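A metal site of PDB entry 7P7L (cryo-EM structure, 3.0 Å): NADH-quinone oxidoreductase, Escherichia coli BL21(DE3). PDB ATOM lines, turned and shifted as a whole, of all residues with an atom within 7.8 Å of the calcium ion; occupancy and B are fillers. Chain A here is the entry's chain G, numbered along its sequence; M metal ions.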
ATOM      1  N   GLU A 614     -16.711 -29.782  24.654  1.00  0.00           N
ATOM      2  CA  GLU A 614     -16.666 -29.856  23.204  1.00  0.00           C
ATOM      3  C   GLU A 614     -17.081 -28.545  22.545  1.00  0.00           C
ATOM      4  O   GLU A 614     -17.453 -28.553  21.364  1.00  0.00           O
ATOM      5  CB  GLU A 614     -17.534 -30.998  22.699  1.00  0.00           C
ATOM      6  CG  GLU A 614     -17.322 -32.313  23.408  1.00  0.00           C
ATOM      7  CD  GLU A 614     -18.515 -32.731  24.233  1.00  0.00           C
ATOM      8  OE1 GLU A 614     -19.453 -31.934  24.360  1.00  0.00           O
ATOM      9  OE2 GLU A 614     -18.511 -33.866  24.754  1.00  0.00           O
ATOM     10  N   SER A 615     -17.047 -27.434  23.270  1.00  0.00           N
ATOM     11  CA  SER A 615     -17.477 -26.174  22.704  1.00  0.00           C
ATOM     12  C   SER A 615     -16.698 -25.023  23.323  1.00  0.00           C
ATOM     13  O   SER A 615     -16.092 -25.159  24.396  1.00  0.00           O
ATOM     14  CB  SER A 615     -18.978 -25.945  22.912  1.00  0.00           C
ATOM     15  OG  SER A 615     -19.263 -25.675  24.264  1.00  0.00           O
ATOM     16  N   ASP A 616     -16.709 -23.902  22.626  1.00  0.00           N
ATOM     17  CA  ASP A 616     -16.165 -22.635  23.105  1.00  0.00           C
ATOM     18  C   ASP A 616     -17.301 -21.703  23.476  1.00  0.00           C
ATOM     19  O   ASP A 616     -18.476 -21.978  23.206  1.00  0.00           O
ATOM     20  CB  ASP A 616     -15.282 -21.990  22.028  1.00  0.00           C
ATOM     21  CG  ASP A 616     -14.438 -22.987  21.295  1.00  0.00           C
ATOM     22  OD1 ASP A 616     -13.521 -23.563  21.921  1.00  0.00           O
ATOM     23  OD2 ASP A 616     -14.686 -23.215  20.094  1.00  0.00           O
ATOM     24  N   GLY A 617     -16.955 -20.601  24.098  1.00  0.00           N
ATOM     25  CA  GLY A 617     -17.959 -19.603  24.413  1.00  0.00           C
ATOM     26  C   GLY A 617     -17.519 -18.717  25.552  1.00  0.00           C
ATOM     27  O   GLY A 617     -16.410 -18.837  26.062  1.00  0.00           O
ATOM     28  N   PHE A 630     -12.741 -22.672  26.271  1.00  0.00           N
ATOM     29  CA  PHE A 630     -12.312 -23.201  24.985  1.00  0.00           C
ATOM     30  C   PHE A 630     -12.652 -24.685  24.884  1.00  0.00           C
ATOM     31  O   PHE A 630     -12.854 -25.362  25.888  1.00  0.00           O
ATOM     32  CB  PHE A 630     -10.810 -22.979  24.776  1.00  0.00           C
ATOM     33  CG  PHE A 630     -10.382 -21.548  24.925  1.00  0.00           C
ATOM     34  CD1 PHE A 630     -10.031 -21.029  26.165  1.00  0.00           C
ATOM     35  CD2 PHE A 630     -10.313 -20.716  23.825  1.00  0.00           C
ATOM     36  CE1 PHE A 630      -9.639 -19.731  26.294  1.00  0.00           C
ATOM     37  CE2 PHE A 630      -9.916 -19.399  23.957  1.00  0.00           C
ATOM     38  CZ  PHE A 630      -9.573 -18.909  25.193  1.00  0.00           C
ATOM     39  N   GLN A 631     -12.709 -25.170  23.643  1.00  0.00           N
ATOM     40  CA  GLN A 631     -12.997 -26.575  23.407  1.00  0.00           C
ATOM     41  C   GLN A 631     -11.811 -27.427  23.833  1.00  0.00           C
ATOM     42  O   GLN A 631     -10.652 -27.095  23.593  1.00  0.00           O
ATOM     43  CB  GLN A 631     -13.298 -26.801  21.930  1.00  0.00           C
ATOM     44  CG  GLN A 631     -13.675 -28.216  21.576  1.00  0.00           C
ATOM     45  CD  GLN A 631     -14.294 -28.327  20.203  1.00  0.00           C
ATOM     46  OE1 GLN A 631     -14.580 -27.318  19.567  1.00  0.00           O
ATOM     47  NE2 GLN A 631     -14.523 -29.550  19.749  1.00  0.00           N
ATOM     48  N   VAL A 632     -12.107 -28.542  24.503  1.00  0.00           N
ATOM     49  CA  VAL A 632     -11.052 -29.453  24.936  1.00  0.00           C
ATOM     50  C   VAL A 632     -10.660 -30.429  23.840  1.00  0.00           C
ATOM     51  O   VAL A 632      -9.479 -30.684  23.628  1.00  0.00           O
ATOM     52  CB  VAL A 632     -11.483 -30.180  26.218  1.00  0.00           C
ATOM     53  CG1 VAL A 632     -10.296 -30.865  26.861  1.00  0.00           C
ATOM     54  CG2 VAL A 632     -12.112 -29.213  27.183  1.00  0.00           C
ATOM     55  N   TYR A 633     -11.634 -30.966  23.119  1.00  0.00           N
ATOM     56  CA  TYR A 633     -11.353 -32.002  22.142  1.00  0.00           C
ATOM     57  C   TYR A 633     -12.403 -31.983  21.056  1.00  0.00           C
ATOM     58  O   TYR A 633     -13.520 -31.481  21.245  1.00  0.00           O
ATOM     59  CB  TYR A 633     -11.312 -33.388  22.805  1.00  0.00           C
ATOM     60  CG  TYR A 633     -12.622 -33.836  23.411  1.00  0.00           C
ATOM     61  CD1 TYR A 633     -13.013 -33.397  24.666  1.00  0.00           C
ATOM     62  CD2 TYR A 633     -13.453 -34.714  22.742  1.00  0.00           C
ATOM     63  CE1 TYR A 633     -14.198 -33.799  25.226  1.00  0.00           C
ATOM     64  CE2 TYR A 633     -14.649 -35.133  23.292  1.00  0.00           C
ATOM     65  CZ  TYR A 633     -15.008 -34.669  24.533  1.00  0.00           C
ATOM     66  OH  TYR A 633     -16.193 -35.071  25.094  1.00  0.00           O
ATOM     67  N   ASP A 634     -12.048 -32.534  19.914  1.00  0.00           N
ATOM     68  CA  ASP A 634     -13.003 -32.719  18.833  1.00  0.00           C
ATOM     69  C   ASP A 634     -13.771 -34.009  19.076  1.00  0.00           C
ATOM     70  O   ASP A 634     -13.156 -35.078  19.203  1.00  0.00           O
ATOM     71  CB  ASP A 634     -12.299 -32.782  17.490  1.00  0.00           C
ATOM     72  CG  ASP A 634     -13.246 -32.634  16.327  1.00  0.00           C
ATOM     73  OD1 ASP A 634     -13.840 -31.548  16.191  1.00  0.00           O
ATOM     74  OD2 ASP A 634     -13.393 -33.601  15.552  1.00  0.00           O
ATOM     75  N   PRO A 635     -15.109 -33.967  19.174  1.00  0.00           N
ATOM     76  CA  PRO A 635     -15.860 -35.199  19.425  1.00  0.00           C
ATOM     77  C   PRO A 635     -15.824 -36.173  18.271  1.00  0.00           C
ATOM     78  O   PRO A 635     -15.911 -37.387  18.501  1.00  0.00           O
ATOM     79  CB  PRO A 635     -17.290 -34.691  19.666  1.00  0.00           C
ATOM     80  CG  PRO A 635     -17.180 -33.216  19.832  1.00  0.00           C
ATOM     81  CD  PRO A 635     -15.973 -32.791  19.076  1.00  0.00           C
ATOM     82  N   LEU A 645     -22.093 -30.342  17.363  1.00  0.00           N
ATOM     83  CA  LEU A 645     -21.606 -28.995  17.117  1.00  0.00           C
ATOM     84  C   LEU A 645     -21.949 -28.073  18.275  1.00  0.00           C
ATOM     85  O   LEU A 645     -22.725 -28.407  19.170  1.00  0.00           O
ATOM     86  CB  LEU A 645     -22.187 -28.446  15.813  1.00  0.00           C
ATOM     87  CG  LEU A 645     -21.680 -29.147  14.555  1.00  0.00           C
ATOM     88  CD1 LEU A 645     -22.412 -28.632  13.343  1.00  0.00           C
ATOM     89  CD2 LEU A 645     -20.180 -28.946  14.416  1.00  0.00           C
ATOM     90  N   GLU A 646     -21.348 -26.883  18.238  1.00  0.00           N
ATOM     91  CA  GLU A 646     -21.645 -25.852  19.212  1.00  0.00           C
ATOM     92  C   GLU A 646     -23.081 -25.377  19.044  1.00  0.00           C
ATOM     93  O   GLU A 646     -23.634 -25.399  17.944  1.00  0.00           O
ATOM     94  CB  GLU A 646     -20.679 -24.681  19.045  1.00  0.00           C
ATOM     95  CG  GLU A 646     -19.236 -24.978  19.418  1.00  0.00           C
ATOM     96  CD  GLU A 646     -18.432 -25.592  18.288  1.00  0.00           C
ATOM     97  OE1 GLU A 646     -18.999 -25.832  17.201  1.00  0.00           O
ATOM     98  OE2 GLU A 646     -17.223 -25.841  18.486  1.00  0.00           O
ATOM     99  N   TRP A 648     -24.256 -22.275  19.476  1.00  0.00           N
ATOM    100  CA  TRP A 648     -24.266 -21.063  18.657  1.00  0.00           C
ATOM    101  C   TRP A 648     -24.021 -21.379  17.192  1.00  0.00           C
ATOM    102  O   TRP A 648     -24.594 -20.727  16.319  1.00  0.00           O
ATOM    103  CB  TRP A 648     -23.223 -20.063  19.160  1.00  0.00           C
ATOM    104  CG  TRP A 648     -21.847 -20.621  19.366  1.00  0.00           C
ATOM    105  CD1 TRP A 648     -21.348 -21.147  20.520  1.00  0.00           C
ATOM    106  CD2 TRP A 648     -20.806 -20.707  18.401  1.00  0.00           C
ATOM    107  NE1 TRP A 648     -20.060 -21.551  20.335  1.00  0.00           N
ATOM    108  CE2 TRP A 648     -19.693 -21.297  19.040  1.00  0.00           C
ATOM    109  CE3 TRP A 648     -20.691 -20.345  17.063  1.00  0.00           C
ATOM    110  CZ2 TRP A 648     -18.491 -21.534  18.379  1.00  0.00           C
ATOM    111  CZ3 TRP A 648     -19.499 -20.590  16.406  1.00  0.00           C
ATOM    112  CH2 TRP A 648     -18.419 -21.175  17.069  1.00  0.00           C
ATOM    113  N   ARG A 649     -23.199 -22.393  16.908  1.00  0.00           N
ATOM    114  CA  ARG A 649     -22.989 -22.806  15.521  1.00  0.00           C
ATOM    115  C   ARG A 649     -24.264 -23.369  14.909  1.00  0.00           C
ATOM    116  O   ARG A 649     -24.618 -23.022  13.772  1.00  0.00           O
ATOM    117  CB  ARG A 649     -21.857 -23.835  15.472  1.00  0.00           C
ATOM    118  CG  ARG A 649     -21.563 -24.387  14.095  1.00  0.00           C
ATOM    119  CD  ARG A 649     -20.121 -24.827  14.007  1.00  0.00           C
ATOM    120  NE  ARG A 649     -19.210 -23.693  14.130  1.00  0.00           N
ATOM    121  CZ  ARG A 649     -17.912 -23.794  14.365  1.00  0.00           C
ATOM    122  NH1 ARG A 649     -17.333 -24.977  14.555  1.00  0.00           N
ATOM    123  NH2 ARG A 649     -17.175 -22.697  14.431  1.00  0.00           N
ATOM    124  N   LEU A 668     -16.335 -18.395  15.887  1.00  0.00           N
ATOM    125  CA  LEU A 668     -16.697 -17.856  17.193  1.00  0.00           C
ATOM    126  C   LEU A 668     -16.497 -16.351  17.271  1.00  0.00           C
ATOM    127  O   LEU A 668     -17.306 -15.641  17.897  1.00  0.00           O
ATOM    128  CB  LEU A 668     -15.874 -18.557  18.281  1.00  0.00           C
ATOM    129  CG  LEU A 668     -16.100 -18.095  19.720  1.00  0.00           C
ATOM    130  CD1 LEU A 668     -17.454 -18.538  20.231  1.00  0.00           C
ATOM    131  CD2 LEU A 668     -14.991 -18.586  20.620  1.00  0.00           C
ATOM    132  N   ARG A 703      -2.757 -27.542  23.070  1.00  0.00           N
ATOM    133  CA  ARG A 703      -3.678 -28.128  24.030  1.00  0.00           C
ATOM    134  C   ARG A 703      -3.030 -29.254  24.844  1.00  0.00           C
ATOM    135  O   ARG A 703      -3.320 -29.387  26.027  1.00  0.00           O
ATOM    136  CB  ARG A 703      -4.920 -28.655  23.319  1.00  0.00           C
ATOM    137  CG  ARG A 703      -6.003 -27.614  23.125  1.00  0.00           C
ATOM    138  CD  ARG A 703      -7.213 -28.217  22.442  1.00  0.00           C
ATOM    139  NE  ARG A 703      -8.324 -27.272  22.386  1.00  0.00           N
ATOM    140  CZ  ARG A 703      -8.561 -26.442  21.381  1.00  0.00           C
ATOM    141  NH1 ARG A 703      -7.782 -26.409  20.321  1.00  0.00           N
ATOM    142  NH2 ARG A 703      -9.614 -25.636  21.452  1.00  0.00           N
ATOM    143  N   GLN A 727      -8.883 -29.224  13.023  1.00  0.00           N
ATOM    144  CA  GLN A 727      -8.565 -27.816  12.825  1.00  0.00           C
ATOM    145  C   GLN A 727      -9.461 -26.963  13.709  1.00  0.00           C
ATOM    146  O   GLN A 727     -10.678 -27.180  13.776  1.00  0.00           O
ATOM    147  CB  GLN A 727      -8.735 -27.421  11.365  1.00  0.00           C
ATOM    148  CG  GLN A 727      -7.766 -28.130  10.429  1.00  0.00           C
ATOM    149  CD  GLN A 727      -6.320 -27.872  10.798  1.00  0.00           C
ATOM    150  OE1 GLN A 727      -5.550 -28.807  11.002  1.00  0.00           O
ATOM    151  NE2 GLN A 727      -5.947 -26.606  10.892  1.00  0.00           N
ATOM    152  N   ASP A 728      -8.857 -26.006  14.408  1.00  0.00           N
ATOM    153  CA  ASP A 728      -9.580 -25.096  15.293  1.00  0.00           C
ATOM    154  C   ASP A 728      -9.613 -23.733  14.629  1.00  0.00           C
ATOM    155  O   ASP A 728      -8.648 -22.972  14.690  1.00  0.00           O
ATOM    156  CB  ASP A 728      -8.899 -25.033  16.658  1.00  0.00           C
ATOM    157  CG  ASP A 728      -9.811 -24.463  17.722  1.00  0.00           C
ATOM    158  OD1 ASP A 728     -11.038 -24.436  17.500  1.00  0.00           O
ATOM    159  OD2 ASP A 728      -9.293 -24.035  18.767  1.00  0.00           O
ATOM    160  N   ILE A 729     -10.740 -23.421  13.982  1.00  0.00           N
ATOM    161  CA  ILE A 729     -10.933 -22.107  13.385  1.00  0.00           C
ATOM    162  C   ILE A 729     -11.503 -21.107  14.372  1.00  0.00           C
ATOM    163  O   ILE A 729     -11.492 -19.896  14.091  1.00  0.00           O
ATOM    164  CB  ILE A 729     -11.834 -22.191  12.151  1.00  0.00           C
ATOM    165  CG1 ILE A 729     -13.248 -22.613  12.559  1.00  0.00           C
ATOM    166  CG2 ILE A 729     -11.268 -23.165  11.137  1.00  0.00           C
ATOM    167  CD1 ILE A 729     -14.248 -22.571  11.434  1.00  0.00           C
ATOM    168  N   ASP A 730     -11.998 -21.567  15.523  1.00  0.00           N
ATOM    169  CA  ASP A 730     -12.659 -20.672  16.461  1.00  0.00           C
ATOM    170  C   ASP A 730     -11.667 -19.957  17.367  1.00  0.00           C
ATOM    171  O   ASP A 730     -11.777 -18.743  17.585  1.00  0.00           O
ATOM    172  CB  ASP A 730     -13.663 -21.448  17.301  1.00  0.00           C
ATOM    173  CG  ASP A 730     -14.673 -22.188  16.461  1.00  0.00           C
ATOM    174  OD1 ASP A 730     -15.176 -21.604  15.493  1.00  0.00           O
ATOM    175  OD2 ASP A 730     -14.962 -23.359  16.781  1.00  0.00           O
ATOM    176  N   THR A 731     -10.683 -20.676  17.913  1.00  0.00           N
ATOM    177  CA  THR A 731      -9.850 -20.160  18.974  1.00  0.00           C
ATOM    178  C   THR A 731      -8.400 -20.079  18.539  1.00  0.00           C
ATOM    179  O   THR A 731      -8.035 -20.415  17.412  1.00  0.00           O
ATOM    180  CB  THR A 731      -9.968 -21.023  20.235  1.00  0.00           C
ATOM    181  OG1 THR A 731      -9.187 -22.203  20.086  1.00  0.00           O
ATOM    182  CG2 THR A 731     -11.410 -21.416  20.497  1.00  0.00           C
ATOM    183  N   PHE A 735      -5.485 -28.440  18.377  1.00  0.00           N
ATOM    184  CA  PHE A 735      -5.723 -29.765  18.937  1.00  0.00           C
ATOM    185  C   PHE A 735      -4.511 -30.658  18.729  1.00  0.00           C
ATOM    186  O   PHE A 735      -4.645 -31.758  18.189  1.00  0.00           O
ATOM    187  CB  PHE A 735      -6.943 -30.411  18.285  1.00  0.00           C
ATOM    188  CG  PHE A 735      -8.236 -29.719  18.582  1.00  0.00           C
ATOM    189  CD1 PHE A 735      -8.895 -29.930  19.777  1.00  0.00           C
ATOM    190  CD2 PHE A 735      -8.799 -28.863  17.658  1.00  0.00           C
ATOM    191  CE1 PHE A 735     -10.090 -29.301  20.036  1.00  0.00           C
ATOM    192  CE2 PHE A 735      -9.992 -28.224  17.918  1.00  0.00           C
ATOM    193  CZ  PHE A 735     -10.637 -28.439  19.115  1.00  0.00           C
HETATM  194 CA    CA M   1     -14.800 -25.128  18.477  1.00  0.00          CA
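The calcium ion is bound by the side-chain amide oxygen of Gln 631 (2.5 Å), the side-chain carboxylate of Asp 730 (2.5 Å), the side-chain carboxylate of Asp 616 (2.5 Å) and the side-chain carboxylate of Glu 646 (2.5 Å).
N of Leu 668 lies within hydrogen-bond range of OD1 of Asp 730 (3.4 Å).
The guanidinium group (NH2) of Arg 703 is in salt-bridge range of the side-chain carboxylate (OD2) of Asp 728 (3.1 Å).
The backbone NH (N) of Gln 631 is in hydrogen-bond range of the backbone carbonyl oxygen (O) of Ser 615 (3.5 Å).
The backbone carbonyl oxygen (O) of Gln 631 is in hydrogen-bond range of the guanidinium group (NE) of Arg 703, at 2.6 Å.
The side-chain carboxylate (OE1) of Glu 646 is in salt-bridge range of the guanidinium group (NH1) of Arg 649 (3.2 Å).
NH2 of Arg 649 is in salt-bridge range of OD1 of Asp 730 (2.5 Å).
NE2 of Gln 631 is in hydrogen-bond range of O of Tyr 633 (2.6 Å).
The backbone carbonyl oxygen (O) of Glu 614 lies close to the side-chain amide nitrogen (NE2) of Gln 631, at 3.5 Å.
Asp 728 touches the calcium ion (OD1 to CA, 3.9 Å).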
